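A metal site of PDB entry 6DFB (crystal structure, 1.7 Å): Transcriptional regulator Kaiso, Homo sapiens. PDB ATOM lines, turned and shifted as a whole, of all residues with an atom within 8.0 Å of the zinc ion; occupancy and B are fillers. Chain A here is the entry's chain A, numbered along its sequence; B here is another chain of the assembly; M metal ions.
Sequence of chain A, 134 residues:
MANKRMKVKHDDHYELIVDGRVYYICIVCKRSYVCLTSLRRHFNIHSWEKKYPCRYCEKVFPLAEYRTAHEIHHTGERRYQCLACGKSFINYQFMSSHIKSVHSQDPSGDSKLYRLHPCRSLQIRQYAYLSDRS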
ATOM      1  N   ASP A  12      -0.173 -24.595  18.608  1.00  0.00           N
ATOM      2  CA  ASP A  12      -1.576 -24.658  18.224  1.00  0.00           C
ATOM      3  C   ASP A  12      -1.878 -25.674  17.118  1.00  0.00           C
ATOM      4  O   ASP A  12      -3.019 -25.793  16.689  1.00  0.00           O
ATOM      5  CB  ASP A  12      -2.045 -23.271  17.776  1.00  0.00           C
ATOM      6  CG  ASP A  12      -1.165 -22.667  16.684  1.00  0.00           C
ATOM      7  OD1 ASP A  12      -0.108 -23.263  16.376  1.00  0.00           O
ATOM      8  OD2 ASP A  12      -1.526 -21.601  16.162  1.00  0.00           O
ATOM      9  N   ILE A  25      -2.949 -29.106  11.082  1.00  0.00           N
ATOM     10  CA  ILE A  25      -4.144 -29.513  11.798  1.00  0.00           C
ATOM     11  C   ILE A  25      -4.302 -28.751  13.106  1.00  0.00           C
ATOM     12  O   ILE A  25      -3.391 -28.745  13.937  1.00  0.00           O
ATOM     13  CB  ILE A  25      -4.108 -31.028  12.131  1.00  0.00           C
ATOM     14  CG1 ILE A  25      -3.709 -31.846  10.904  1.00  0.00           C
ATOM     15  CG2 ILE A  25      -5.455 -31.487  12.676  1.00  0.00           C
ATOM     16  CD1 ILE A  25      -4.627 -31.675   9.721  1.00  0.00           C
ATOM     17  N   CYS A  26      -5.433 -28.089  13.298  1.00  0.00           N
ATOM     18  CA  CYS A  26      -5.698 -27.419  14.559  1.00  0.00           C
ATOM     19  C   CYS A  26      -5.712 -28.427  15.705  1.00  0.00           C
ATOM     20  O   CYS A  26      -6.416 -29.425  15.666  1.00  0.00           O
ATOM     21  CB  CYS A  26      -7.034 -26.683  14.492  1.00  0.00           C
ATOM     22  SG  CYS A  26      -7.490 -25.954  16.061  1.00  0.00           S
ATOM     23  N   ILE A  27      -4.901 -28.160  16.739  1.00  0.00           N
ATOM     24  CA  ILE A  27      -4.801 -29.079  17.860  1.00  0.00           C
ATOM     25  C   ILE A  27      -6.076 -29.087  18.715  1.00  0.00           C
ATOM     26  O   ILE A  27      -6.326 -30.020  19.469  1.00  0.00           O
ATOM     27  CB  ILE A  27      -3.572 -28.731  18.748  1.00  0.00           C
ATOM     28  CG1 ILE A  27      -3.245 -29.884  19.696  1.00  0.00           C
ATOM     29  CG2 ILE A  27      -3.803 -27.438  19.513  1.00  0.00           C
ATOM     30  CD1 ILE A  27      -3.292 -31.247  19.031  1.00  0.00           C
ATOM     31  N   VAL A  28      -6.918 -28.058  18.575  1.00  0.00           N
ATOM     32  CA  VAL A  28      -8.145 -27.990  19.370  1.00  0.00           C
ATOM     33  C   VAL A  28      -9.332 -28.691  18.699  1.00  0.00           C
ATOM     34  O   VAL A  28     -10.003 -29.510  19.334  1.00  0.00           O
ATOM     35  CB  VAL A  28      -8.530 -26.513  19.656  1.00  0.00           C
ATOM     36  CG1 VAL A  28      -9.899 -26.445  20.328  1.00  0.00           C
ATOM     37  CG2 VAL A  28      -7.480 -25.845  20.524  1.00  0.00           C
ATOM     38  N   CYS A  29      -9.596 -28.376  17.426  1.00  0.00           N
ATOM     39  CA  CYS A  29     -10.808 -28.868  16.742  1.00  0.00           C
ATOM     40  C   CYS A  29     -10.502 -29.799  15.568  1.00  0.00           C
ATOM     41  O   CYS A  29     -11.421 -30.349  14.949  1.00  0.00           O
ATOM     42  CB  CYS A  29     -11.662 -27.679  16.250  1.00  0.00           C
ATOM     43  SG  CYS A  29     -11.046 -26.748  14.820  1.00  0.00           S
ATOM     44  N   LYS A  30      -9.222 -29.981  15.274  1.00  0.00           N
ATOM     45  CA  LYS A  30      -8.736 -30.903  14.239  1.00  0.00           C
ATOM     46  C   LYS A  30      -9.105 -30.491  12.805  1.00  0.00           C
ATOM     47  O   LYS A  30      -9.093 -31.323  11.897  1.00  0.00           O
ATOM     48  CB  LYS A  30      -9.229 -32.335  14.497  1.00  0.00           C
ATOM     49  CG  LYS A  30      -8.268 -33.183  15.326  1.00  0.00           C
ATOM     50  CD  LYS A  30      -8.126 -32.665  16.747  1.00  0.00           C
ATOM     51  CE  LYS A  30      -7.185 -33.545  17.551  1.00  0.00           C
ATOM     52  NZ  LYS A  30      -7.032 -33.047  18.949  1.00  0.00           N
ATOM     53  N   ARG A  31      -9.435 -29.214  12.586  1.00  0.00           N
ATOM     54  CA  ARG A  31      -9.649 -28.741  11.230  1.00  0.00           C
ATOM     55  C   ARG A  31      -8.329 -28.719  10.472  1.00  0.00           C
ATOM     56  O   ARG A  31      -7.286 -28.440  11.055  1.00  0.00           O
ATOM     57  CB  ARG A  31     -10.314 -27.350  11.219  1.00  0.00           C
ATOM     58  CG  ARG A  31     -11.830 -27.382  11.332  1.00  0.00           C
ATOM     59  CD  ARG A  31     -12.414 -25.959  11.328  1.00  0.00           C
ATOM     60  NE  ARG A  31     -13.829 -25.953  10.956  1.00  0.00           N
ATOM     61  CZ  ARG A  31     -14.835 -26.085  11.803  1.00  0.00           C
ATOM     62  NH1 ARG A  31     -14.597 -26.262  13.102  1.00  0.00           N
ATOM     63  NH2 ARG A  31     -16.090 -26.056  11.362  1.00  0.00           N
ATOM     64  N   SER A  32      -8.380 -29.009   9.174  1.00  0.00           N
ATOM     65  CA  SER A  32      -7.177 -29.094   8.357  1.00  0.00           C
ATOM     66  C   SER A  32      -6.975 -27.845   7.501  1.00  0.00           C
ATOM     67  O   SER A  32      -7.929 -27.317   6.955  1.00  0.00           O
ATOM     68  CB  SER A  32      -7.255 -30.326   7.463  1.00  0.00           C
ATOM     69  OG  SER A  32      -6.165 -30.372   6.553  1.00  0.00           O
ATOM     70  N   TYR A  33      -5.726 -27.373   7.390  1.00  0.00           N
ATOM     71  CA  TYR A  33      -5.419 -26.186   6.583  1.00  0.00           C
ATOM     72  C   TYR A  33      -4.220 -26.433   5.673  1.00  0.00           C
ATOM     73  O   TYR A  33      -3.245 -27.083   6.057  1.00  0.00           O
ATOM     74  CB  TYR A  33      -5.167 -24.981   7.505  1.00  0.00           C
ATOM     75  CG  TYR A  33      -6.399 -24.673   8.312  1.00  0.00           C
ATOM     76  CD1 TYR A  33      -6.610 -25.277   9.541  1.00  0.00           C
ATOM     77  CD2 TYR A  33      -7.369 -23.824   7.806  1.00  0.00           C
ATOM     78  CE1 TYR A  33      -7.760 -25.027  10.259  1.00  0.00           C
ATOM     79  CE2 TYR A  33      -8.516 -23.563   8.515  1.00  0.00           C
ATOM     80  CZ  TYR A  33      -8.714 -24.152   9.732  1.00  0.00           C
ATOM     81  OH  TYR A  33      -9.852 -23.912  10.443  1.00  0.00           O
ATOM     82  N   LEU A  39      -4.482 -21.410   9.529  1.00  0.00           N
ATOM     83  CA  LEU A  39      -4.636 -22.016  10.841  1.00  0.00           C
ATOM     84  C   LEU A  39      -4.534 -20.936  11.918  1.00  0.00           C
ATOM     85  O   LEU A  39      -5.344 -20.910  12.842  1.00  0.00           O
ATOM     86  CB  LEU A  39      -3.585 -23.117  11.052  1.00  0.00           C
ATOM     87  CG  LEU A  39      -3.543 -23.976  12.321  1.00  0.00           C
ATOM     88  CD1 LEU A  39      -4.808 -23.964  13.135  1.00  0.00           C
ATOM     89  CD2 LEU A  39      -3.243 -25.409  11.899  1.00  0.00           C
ATOM     90  N   HIS A  42      -7.664 -18.838  11.828  1.00  0.00           N
ATOM     91  CA  HIS A  42      -8.705 -19.668  12.455  1.00  0.00           C
ATOM     92  C   HIS A  42      -8.581 -19.776  13.975  1.00  0.00           C
ATOM     93  O   HIS A  42      -9.586 -19.702  14.695  1.00  0.00           O
ATOM     94  CB  HIS A  42      -8.667 -21.076  11.865  1.00  0.00           C
ATOM     95  CG  HIS A  42      -9.294 -22.106  12.761  1.00  0.00           C
ATOM     96  ND1 HIS A  42     -10.654 -22.227  12.912  1.00  0.00           N
ATOM     97  CD2 HIS A  42      -8.744 -23.045  13.570  1.00  0.00           C
ATOM     98  CE1 HIS A  42     -10.921 -23.190  13.763  1.00  0.00           C
ATOM     99  NE2 HIS A  42      -9.781 -23.697  14.190  1.00  0.00           N
ATOM    100  N   PHE A  43      -7.360 -19.981  14.460  1.00  0.00           N
ATOM    101  CA  PHE A  43      -7.157 -20.368  15.853  1.00  0.00           C
ATOM    102  C   PHE A  43      -7.622 -19.303  16.832  1.00  0.00           C
ATOM    103  O   PHE A  43      -7.891 -19.594  17.987  1.00  0.00           O
ATOM    104  CB  PHE A  43      -5.679 -20.709  16.115  1.00  0.00           C
ATOM    105  CG  PHE A  43      -5.454 -21.515  17.378  1.00  0.00           C
ATOM    106  CD1 PHE A  43      -5.618 -22.887  17.364  1.00  0.00           C
ATOM    107  CD2 PHE A  43      -5.057 -20.899  18.556  1.00  0.00           C
ATOM    108  CE1 PHE A  43      -5.402 -23.650  18.534  1.00  0.00           C
ATOM    109  CE2 PHE A  43      -4.856 -21.641  19.712  1.00  0.00           C
ATOM    110  CZ  PHE A  43      -5.021 -23.018  19.689  1.00  0.00           C
ATOM    111  N   ASN A  44      -7.751 -18.058  16.357  1.00  0.00           N
ATOM    112  CA  ASN A  44      -8.209 -16.979  17.225  1.00  0.00           C
ATOM    113  C   ASN A  44      -9.627 -17.241  17.745  1.00  0.00           C
ATOM    114  O   ASN A  44     -10.011 -16.716  18.787  1.00  0.00           O
ATOM    115  CB  ASN A  44      -8.171 -15.638  16.491  1.00  0.00           C
ATOM    116  CG  ASN A  44      -8.141 -14.458  17.440  1.00  0.00           C
ATOM    117  OD1 ASN A  44      -7.352 -14.425  18.398  1.00  0.00           O
ATOM    118  ND2 ASN A  44      -9.005 -13.472  17.196  1.00  0.00           N
ATOM    119  N   ILE A  45     -10.390 -18.030  17.000  1.00  0.00           N
ATOM    120  CA  ILE A  45     -11.721 -18.447  17.426  1.00  0.00           C
ATOM    121  C   ILE A  45     -11.642 -19.190  18.768  1.00  0.00           C
ATOM    122  O   ILE A  45     -12.509 -19.067  19.626  1.00  0.00           O
ATOM    123  CB  ILE A  45     -12.392 -19.336  16.373  1.00  0.00           C
ATOM    124  CG1 ILE A  45     -12.659 -18.531  15.091  1.00  0.00           C
ATOM    125  CG2 ILE A  45     -13.691 -19.933  16.891  1.00  0.00           C
ATOM    126  CD1 ILE A  45     -13.138 -19.370  13.934  1.00  0.00           C
ATOM    127  N   HIS A  46     -10.560 -19.960  18.945  1.00  0.00           N
ATOM    128  CA  HIS A  46     -10.364 -20.681  20.198  1.00  0.00           C
ATOM    129  C   HIS A  46      -9.748 -19.789  21.291  1.00  0.00           C
ATOM    130  O   HIS A  46     -10.246 -19.758  22.419  1.00  0.00           O
ATOM    131  CB  HIS A  46      -9.456 -21.899  19.986  1.00  0.00           C
ATOM    132  CG  HIS A  46      -9.965 -22.842  18.933  1.00  0.00           C
ATOM    133  ND1 HIS A  46     -11.284 -23.256  18.872  1.00  0.00           N
ATOM    134  CD2 HIS A  46      -9.337 -23.443  17.899  1.00  0.00           C
ATOM    135  CE1 HIS A  46     -11.432 -24.073  17.843  1.00  0.00           C
ATOM    136  NE2 HIS A  46     -10.272 -24.210  17.241  1.00  0.00           N
ATOM    137  P    DT B   8     -12.158 -23.388   7.653  1.00  0.00           P
ATOM    138  OP1  DT B   8     -12.220 -24.881   7.705  1.00  0.00           O
ATOM    139  OP2  DT B   8     -11.706 -22.643   8.843  1.00  0.00           O
ATOM    140  O5'  DT B   8     -11.215 -22.981   6.450  1.00  0.00           O
ATOM    141  C5'  DT B   8     -11.295 -23.675   5.201  1.00  0.00           C
ATOM    142  C4'  DT B   8     -10.500 -22.971   4.118  1.00  0.00           C
ATOM    143  O4'  DT B   8     -11.163 -21.723   3.703  1.00  0.00           O
ATOM    144  C3'  DT B   8      -9.067 -22.577   4.469  1.00  0.00           C
ATOM    145  O3'  DT B   8      -8.287 -22.723   3.313  1.00  0.00           O
ATOM    146  C2'  DT B   8      -9.222 -21.094   4.816  1.00  0.00           C
ATOM    147  C1'  DT B   8     -10.197 -20.686   3.714  1.00  0.00           C
ATOM    148  N1   DT B   8     -10.925 -19.378   3.894  1.00  0.00           N
ATOM    149  C2   DT B   8     -11.475 -18.807   2.783  1.00  0.00           C
ATOM    150  O2   DT B   8     -11.354 -19.295   1.675  1.00  0.00           O
ATOM    151  N3   DT B   8     -12.153 -17.637   2.997  1.00  0.00           N
ATOM    152  C4   DT B   8     -12.348 -17.004   4.191  1.00  0.00           C
ATOM    153  O4   DT B   8     -12.981 -15.937   4.265  1.00  0.00           O
ATOM    154  C5   DT B   8     -11.753 -17.640   5.345  1.00  0.00           C
ATOM    155  C7   DT B   8     -11.904 -17.028   6.712  1.00  0.00           C
ATOM    156  C6   DT B   8     -11.086 -18.819   5.152  1.00  0.00           C
HETATM  157 ZN    ZN M   1      -9.616 -25.196  15.579  1.00  0.00          ZN
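Four residues have an atom within 4 Å of the zinc ion: Cys 26, Cys 29, His 42 and His 46.
The nearest printed residue that does not touch the zinc ion is Val 28 (4.4 Å).
The backbone NH (N) of Cys 26 sits at hydrogen-bond distance from the backbone carbonyl oxygen (O) of Arg 31, at 2.9 Å.
The side-chain sulfur of Cys 29 sits close to the backbone NH of Arg 31 (3.7 Å).
SG of Cys 26 lies close to N of Val 28, at 3.3 Å.
A ring nitrogen (ND1) of His 42 lies close to the side-chain hydroxyl (OH) of Tyr 33 (3.1 Å).
The zinc ion is bound by a ring nitrogen (NE2) of His 46 (2.0 Å).
The zinc ion is bound by a ring nitrogen (NE2) of His 42 (2.1 Å).
SG of Cys 29 is bound to the zinc ion, at 2.2 Å.
The zinc ion is bound by SG of Cys 26 (2.3 Å).
The zinc ion has four donor atoms within binding distance.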
